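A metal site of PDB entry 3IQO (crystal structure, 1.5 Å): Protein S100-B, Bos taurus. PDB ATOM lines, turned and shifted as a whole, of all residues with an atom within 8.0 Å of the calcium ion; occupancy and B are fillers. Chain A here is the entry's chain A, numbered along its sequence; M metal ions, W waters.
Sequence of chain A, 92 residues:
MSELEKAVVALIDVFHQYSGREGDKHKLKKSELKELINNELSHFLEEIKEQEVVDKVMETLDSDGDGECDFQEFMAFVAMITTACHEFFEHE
The side-chain hydroxyl (OG) of Ser 19 lies within hydrogen-bond range of the backbone carbonyl oxygen (O) of Lys 25, at 2.8 Å.
NZ of Lys 27 lies within salt-bridge range of OD2 of Asp 24 (2.8 Å).
The side-chain hydroxyl (OG) of Ser 19 is in hydrogen-bond range of the backbone carbonyl oxygen (O) of Phe 15 (3.0 Å).
OD1 of Asp 24 sits at hydrogen-bond distance from N of His 26, 2.8 Å away.
The side-chain carboxylate of Glu 32 sits close to the backbone NH of Arg 21 (3.3 Å).
The backbone NH (N) of Lys 29 lies close to the side-chain carboxylate (OE1) of Glu 32, at 2.9 Å.
Five residues have an atom within 4 Å of the calcium ion: Ser 19, Glu 22, Asp 24, Lys 27 and Glu 32.
The nearest printed residue that does not touch the calcium ion is Gly 23 (4.3 Å).
The backbone carbonyl oxygen (O) of Asp 24 is bound to the calcium ion (2.3 Å).
O of Ser 19 is bound to the calcium ion.
The calcium ion is bound by the backbone carbonyl oxygen (O) of Glu 22 (2.4 Å).
The calcium ion is bound by the backbone carbonyl oxygen (O) of Lys 27 (2.4 Å).
The calcium ion is bound by the side-chain carboxylate (OE1) of Glu 32 (2.5 Å).
The calcium ion is bound by water W1 (2.6 Å).
The side-chain carboxylate (OE2) of Glu 32 is bound to the calcium ion (2.6 Å).
The calcium ion has seven donor atoms within binding distance.
Water W1 lies within hydrogen-bond range of the side-chain carboxylate of Glu 68 (2.6 Å) and the side-chain amino group of Lys 29 (3.1 Å).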
ATOM      1  N   PHE A  15     -16.260 -22.873  -4.078  1.00  0.00           N
ATOM      2  CA  PHE A  15     -16.281 -21.764  -3.092  1.00  0.00           C
ATOM      3  C   PHE A  15     -16.774 -20.478  -3.734  1.00  0.00           C
ATOM      4  O   PHE A  15     -17.611 -19.768  -3.183  1.00  0.00           O
ATOM      5  CB  PHE A  15     -14.919 -21.534  -2.460  1.00  0.00           C
ATOM      6  CG  PHE A  15     -14.908 -20.395  -1.488  1.00  0.00           C
ATOM      7  CD1 PHE A  15     -15.322 -20.588  -0.167  1.00  0.00           C
ATOM      8  CD2 PHE A  15     -14.511 -19.110  -1.874  1.00  0.00           C
ATOM      9  CE1 PHE A  15     -15.327 -19.536   0.745  1.00  0.00           C
ATOM     10  CE2 PHE A  15     -14.514 -18.045  -0.980  1.00  0.00           C
ATOM     11  CZ  PHE A  15     -14.945 -18.255   0.343  1.00  0.00           C
ATOM     12  N   HIS A  16     -16.246 -20.191  -4.908  1.00  0.00           N
ATOM     13  CA  HIS A  16     -16.618 -18.988  -5.596  1.00  0.00           C
ATOM     14  C   HIS A  16     -18.053 -18.960  -6.138  1.00  0.00           C
ATOM     15  O   HIS A  16     -18.673 -17.889  -6.187  1.00  0.00           O
ATOM     16  CB  HIS A  16     -15.577 -18.729  -6.634  1.00  0.00           C
ATOM     17  CG  HIS A  16     -14.384 -18.009  -6.079  1.00  0.00           C
ATOM     18  ND1 HIS A  16     -13.095 -18.236  -6.517  1.00  0.00           N
ATOM     19  CD2 HIS A  16     -14.289 -17.063  -5.114  1.00  0.00           C
ATOM     20  CE1 HIS A  16     -12.271 -17.447  -5.861  1.00  0.00           C
ATOM     21  NE2 HIS A  16     -12.964 -16.737  -4.995  1.00  0.00           N
ATOM     22  N   GLN A  17     -18.577 -20.130  -6.515  1.00  0.00           N
ATOM     23  CA  GLN A  17     -19.980 -20.228  -6.968  1.00  0.00           C
ATOM     24  C   GLN A  17     -20.858 -19.744  -5.818  1.00  0.00           C
ATOM     25  O   GLN A  17     -21.803 -18.957  -6.022  1.00  0.00           O
ATOM     26  CB  GLN A  17     -20.419 -21.677  -7.293  1.00  0.00           C
ATOM     27  CG  GLN A  17     -19.702 -22.456  -8.380  1.00  0.00           C
ATOM     28  CD  GLN A  17     -19.584 -21.724  -9.691  1.00  0.00           C
ATOM     29  OE1 GLN A  17     -20.578 -21.462 -10.367  1.00  0.00           O
ATOM     30  NE2 GLN A  17     -18.349 -21.412 -10.076  1.00  0.00           N
ATOM     31  N   TYR A  18     -20.586 -20.240  -4.622  1.00  0.00           N
ATOM     32  CA  TYR A  18     -21.428 -19.934  -3.477  1.00  0.00           C
ATOM     33  C   TYR A  18     -21.129 -18.606  -2.803  1.00  0.00           C
ATOM     34  O   TYR A  18     -22.061 -17.874  -2.433  1.00  0.00           O
ATOM     35  CB  TYR A  18     -21.473 -21.105  -2.479  1.00  0.00           C
ATOM     36  CG  TYR A  18     -22.295 -22.238  -3.034  1.00  0.00           C
ATOM     37  CD1 TYR A  18     -21.745 -23.185  -3.914  1.00  0.00           C
ATOM     38  CD2 TYR A  18     -23.642 -22.321  -2.740  1.00  0.00           C
ATOM     39  CE1 TYR A  18     -22.549 -24.205  -4.445  1.00  0.00           C
ATOM     40  CE2 TYR A  18     -24.424 -23.324  -3.251  1.00  0.00           C
ATOM     41  CZ  TYR A  18     -23.888 -24.245  -4.091  1.00  0.00           C
ATOM     42  OH  TYR A  18     -24.714 -25.197  -4.596  1.00  0.00           O
ATOM     43  N   SER A  19     -19.859 -18.258  -2.673  1.00  0.00           N
ATOM     44  CA  SER A  19     -19.497 -17.014  -2.010  1.00  0.00           C
ATOM     45  C   SER A  19     -19.990 -15.785  -2.801  1.00  0.00           C
ATOM     46  O   SER A  19     -20.260 -14.729  -2.216  1.00  0.00           O
ATOM     47  CB  SER A  19     -17.967 -16.946  -1.779  1.00  0.00           C
ATOM     48  OG  SER A  19     -17.255 -16.786  -2.981  1.00  0.00           O
ATOM     49  N   GLY A  20     -20.111 -15.932  -4.125  1.00  0.00           N
ATOM     50  CA  GLY A  20     -20.429 -14.824  -5.001  1.00  0.00           C
ATOM     51  C   GLY A  20     -21.896 -14.445  -5.068  1.00  0.00           C
ATOM     52  O   GLY A  20     -22.259 -13.492  -5.756  1.00  0.00           O
ATOM     53  N   ARG A  21     -22.738 -15.204  -4.366  1.00  0.00           N
ATOM     54  CA  ARG A  21     -24.205 -15.010  -4.492  1.00  0.00           C
ATOM     55  C   ARG A  21     -24.711 -13.715  -3.919  1.00  0.00           C
ATOM     56  O   ARG A  21     -25.481 -12.997  -4.566  1.00  0.00           O
ATOM     57  CB  ARG A  21     -24.955 -16.165  -3.840  1.00  0.00           C
ATOM     58  CG  ARG A  21     -24.819 -17.420  -4.623  1.00  0.00           C
ATOM     59  CD  ARG A  21     -25.459 -18.582  -3.906  1.00  0.00           C
ATOM     60  NE  ARG A  21     -25.506 -19.770  -4.750  1.00  0.00           N
ATOM     61  CZ  ARG A  21     -26.359 -20.772  -4.563  1.00  0.00           C
ATOM     62  NH1 ARG A  21     -27.211 -20.746  -3.548  1.00  0.00           N
ATOM     63  NH2 ARG A  21     -26.332 -21.816  -5.383  1.00  0.00           N
ATOM     64  N   GLU A  22     -24.277 -13.422  -2.699  1.00  0.00           N
ATOM     65  CA  GLU A  22     -24.745 -12.257  -1.956  1.00  0.00           C
ATOM     66  C   GLU A  22     -23.617 -11.614  -1.146  1.00  0.00           C
ATOM     67  O   GLU A  22     -22.605 -12.261  -0.843  1.00  0.00           O
ATOM     68  CB  GLU A  22     -25.850 -12.690  -0.992  1.00  0.00           C
ATOM     69  CG  GLU A  22     -27.132 -13.190  -1.665  1.00  0.00           C
ATOM     70  CD  GLU A  22     -28.185 -13.677  -0.663  1.00  0.00           C
ATOM     71  OE1 GLU A  22     -28.274 -13.100   0.453  1.00  0.00           O
ATOM     72  OE2 GLU A  22     -28.946 -14.625  -0.975  1.00  0.00           O
ATOM     73  N   GLY A  23     -23.798 -10.354  -0.788  1.00  0.00           N
ATOM     74  CA  GLY A  23     -22.882  -9.653   0.103  1.00  0.00           C
ATOM     75  C   GLY A  23     -21.454  -9.720  -0.401  1.00  0.00           C
ATOM     76  O   GLY A  23     -21.198  -9.551  -1.592  1.00  0.00           O
ATOM     77  N   ASP A  24     -20.528  -9.981   0.520  1.00  0.00           N
ATOM     78  CA  ASP A  24     -19.133 -10.094   0.154  1.00  0.00           C
ATOM     79  C   ASP A  24     -19.023 -11.211  -0.864  1.00  0.00           C
ATOM     80  O   ASP A  24     -19.483 -12.344  -0.600  1.00  0.00           O
ATOM     81  CB  ASP A  24     -18.290 -10.403   1.394  1.00  0.00           C
ATOM     82  CG  ASP A  24     -16.797 -10.282   1.142  1.00  0.00           C
ATOM     83  OD1 ASP A  24     -16.321 -10.546   0.007  1.00  0.00           O
ATOM     84  OD2 ASP A  24     -16.068  -9.875   2.083  1.00  0.00           O
ATOM     85  N   LYS A  25     -18.456 -10.910  -2.036  1.00  0.00           N
ATOM     86  CA  LYS A  25     -18.376 -11.962  -3.058  1.00  0.00           C
ATOM     87  C   LYS A  25     -17.258 -12.971  -2.802  1.00  0.00           C
ATOM     88  O   LYS A  25     -17.200 -13.985  -3.485  1.00  0.00           O
ATOM     89  CB  LYS A  25     -18.334 -11.407  -4.495  1.00  0.00           C
ATOM     90  CG  LYS A  25     -17.060 -10.755  -4.926  1.00  0.00           C
ATOM     91  CD  LYS A  25     -17.149 -10.374  -6.386  1.00  0.00           C
ATOM     92  CE  LYS A  25     -15.930  -9.594  -6.805  1.00  0.00           C
ATOM     93  NZ  LYS A  25     -16.032  -9.129  -8.227  1.00  0.00           N
ATOM     94  N   HIS A  26     -16.429 -12.713  -1.779  1.00  0.00           N
ATOM     95  CA  HIS A  26     -15.333 -13.633  -1.436  1.00  0.00           C
ATOM     96  C   HIS A  26     -15.488 -14.348  -0.072  1.00  0.00           C
ATOM     97  O   HIS A  26     -14.542 -14.987   0.426  1.00  0.00           O
ATOM     98  CB  HIS A  26     -13.974 -12.958  -1.563  1.00  0.00           C
ATOM     99  CG  HIS A  26     -13.785 -12.309  -2.901  1.00  0.00           C
ATOM    100  ND1 HIS A  26     -13.784 -13.045  -4.076  1.00  0.00           N
ATOM    101  CD2 HIS A  26     -13.677 -11.014  -3.272  1.00  0.00           C
ATOM    102  CE1 HIS A  26     -13.638 -12.234  -5.097  1.00  0.00           C
ATOM    103  NE2 HIS A  26     -13.574 -10.992  -4.641  1.00  0.00           N
ATOM    104  N   LYS A  27     -16.669 -14.233   0.523  1.00  0.00           N
ATOM    105  CA  LYS A  27     -16.958 -14.941   1.763  1.00  0.00           C
ATOM    106  C   LYS A  27     -18.334 -15.549   1.682  1.00  0.00           C
ATOM    107  O   LYS A  27     -19.210 -15.027   0.964  1.00  0.00           O
ATOM    108  CB  LYS A  27     -16.875 -14.021   2.976  1.00  0.00           C
ATOM    109  CG  LYS A  27     -15.525 -13.324   3.121  1.00  0.00           C
ATOM    110  CD  LYS A  27     -15.327 -12.710   4.479  1.00  0.00           C
ATOM    111  CE  LYS A  27     -13.981 -12.013   4.556  1.00  0.00           C
ATOM    112  NZ  LYS A  27     -13.947 -10.796   3.681  1.00  0.00           N
ATOM    113  N   LEU A  28     -18.528 -16.633   2.435  1.00  0.00           N
ATOM    114  CA  LEU A  28     -19.826 -17.304   2.582  1.00  0.00           C
ATOM    115  C   LEU A  28     -20.559 -16.779   3.821  1.00  0.00           C
ATOM    116  O   LEU A  28     -20.088 -16.918   4.959  1.00  0.00           O
ATOM    117  CB  LEU A  28     -19.663 -18.820   2.735  1.00  0.00           C
ATOM    118  CG  LEU A  28     -19.005 -19.573   1.579  1.00  0.00           C
ATOM    119  CD1 LEU A  28     -18.522 -20.951   2.091  1.00  0.00           C
ATOM    120  CD2 LEU A  28     -19.927 -19.780   0.384  1.00  0.00           C
ATOM    121  N   LYS A  29     -21.713 -16.173   3.603  1.00  0.00           N
ATOM    122  CA  LYS A  29     -22.632 -15.839   4.695  1.00  0.00           C
ATOM    123  C   LYS A  29     -23.394 -17.150   5.073  1.00  0.00           C
ATOM    124  O   LYS A  29     -23.306 -18.166   4.379  1.00  0.00           O
ATOM    125  CB  LYS A  29     -23.588 -14.697   4.272  1.00  0.00           C
ATOM    126  CG  LYS A  29     -24.525 -15.057   3.092  1.00  0.00           C
ATOM    127  CD  LYS A  29     -25.666 -14.036   2.758  1.00  0.00           C
ATOM    128  CE  LYS A  29     -25.348 -12.628   3.159  1.00  0.00           C
ATOM    129  NZ  LYS A  29     -24.359 -11.992   2.245  1.00  0.00           N
ATOM    130  N   LYS A  30     -24.137 -17.113   6.167  1.00  0.00           N
ATOM    131  CA  LYS A  30     -24.880 -18.331   6.555  1.00  0.00           C
ATOM    132  C   LYS A  30     -25.752 -18.955   5.464  1.00  0.00           C
ATOM    133  O   LYS A  30     -25.713 -20.200   5.293  1.00  0.00           O
ATOM    134  CB  LYS A  30     -25.782 -18.042   7.765  1.00  0.00           C
ATOM    135  CG  LYS A  30     -25.049 -17.896   9.071  1.00  0.00           C
ATOM    136  CD  LYS A  30     -26.020 -17.468  10.154  1.00  0.00           C
ATOM    137  CE  LYS A  30     -25.315 -17.344  11.469  1.00  0.00           C
ATOM    138  NZ  LYS A  30     -26.247 -16.860  12.525  1.00  0.00           N
ATOM    139  N   SER A  31     -26.561 -18.146   4.769  1.00  0.00           N
ATOM    140  CA  SER A  31     -27.422 -18.701   3.702  1.00  0.00           C
ATOM    141  C   SER A  31     -26.598 -19.370   2.594  1.00  0.00           C
ATOM    142  O   SER A  31     -26.990 -20.430   2.060  1.00  0.00           O
ATOM    143  CB  SER A  31     -28.357 -17.641   3.121  1.00  0.00           C
ATOM    144  OG  SER A  31     -27.621 -16.605   2.525  1.00  0.00           O
ATOM    145  N   GLU A  32     -25.452 -18.784   2.254  1.00  0.00           N
ATOM    146  CA  GLU A  32     -24.607 -19.373   1.196  1.00  0.00           C
ATOM    147  C   GLU A  32     -23.958 -20.689   1.652  1.00  0.00           C
ATOM    148  O   GLU A  32     -23.890 -21.665   0.891  1.00  0.00           O
ATOM    149  CB  GLU A  32     -23.536 -18.375   0.752  1.00  0.00           C
ATOM    150  CG  GLU A  32     -24.072 -17.142   0.011  1.00  0.00           C
ATOM    151  CD  GLU A  32     -23.017 -16.026  -0.119  1.00  0.00           C
ATOM    152  OE1 GLU A  32     -22.082 -15.955   0.725  1.00  0.00           O
ATOM    153  OE2 GLU A  32     -23.118 -15.210  -1.069  1.00  0.00           O
ATOM    154  N   LEU A  33     -23.487 -20.724   2.895  1.00  0.00           N
ATOM    155  CA  LEU A  33     -22.876 -21.934   3.481  1.00  0.00           C
ATOM    156  C   LEU A  33     -23.944 -23.045   3.591  1.00  0.00           C
ATOM    157  O   LEU A  33     -23.680 -24.202   3.271  1.00  0.00           O
ATOM    158  CB  LEU A  33     -22.282 -21.570   4.852  1.00  0.00           C
ATOM    159  CG  LEU A  33     -21.758 -22.747   5.689  1.00  0.00           C
ATOM    160  CD1 LEU A  33     -20.575 -23.388   4.974  1.00  0.00           C
ATOM    161  CD2 LEU A  33     -21.379 -22.268   7.070  1.00  0.00           C
ATOM    162  N   GLU A  68     -18.694 -14.789   8.933  1.00  0.00           N
ATOM    163  CA  GLU A  68     -18.714 -15.315   7.572  1.00  0.00           C
ATOM    164  C   GLU A  68     -17.577 -16.301   7.406  1.00  0.00           C
ATOM    165  O   GLU A  68     -16.653 -16.319   8.211  1.00  0.00           O
ATOM    166  CB  GLU A  68     -18.583 -14.200   6.517  1.00  0.00           C
ATOM    167  CG  GLU A  68     -19.751 -13.196   6.549  1.00  0.00           C
ATOM    168  CD  GLU A  68     -20.051 -12.602   5.194  1.00  0.00           C
ATOM    169  OE1 GLU A  68     -19.777 -13.250   4.153  1.00  0.00           O
ATOM    170  OE2 GLU A  68     -20.605 -11.484   5.157  1.00  0.00           O
ATOM    171  N   CYS A  69     -17.664 -17.142   6.380  1.00  0.00           N
ATOM    172  CA  CYS A  69     -16.652 -18.148   6.132  1.00  0.00           C
ATOM    173  C   CYS A  69     -15.803 -17.702   4.926  1.00  0.00           C
ATOM    174  O   CYS A  69     -16.299 -17.625   3.790  1.00  0.00           O
ATOM    175  CB  CYS A  69     -17.320 -19.522   5.887  1.00  0.00           C
ATOM    176  SG  CYS A  69     -16.143 -20.870   5.619  1.00  0.00           S
HETATM  177 CA    CA M   1     -21.028 -13.949  -0.229  1.00  0.00          CA
HETATM  178  O   HOH W   1     -21.415 -13.085   2.139  1.00  0.00           O
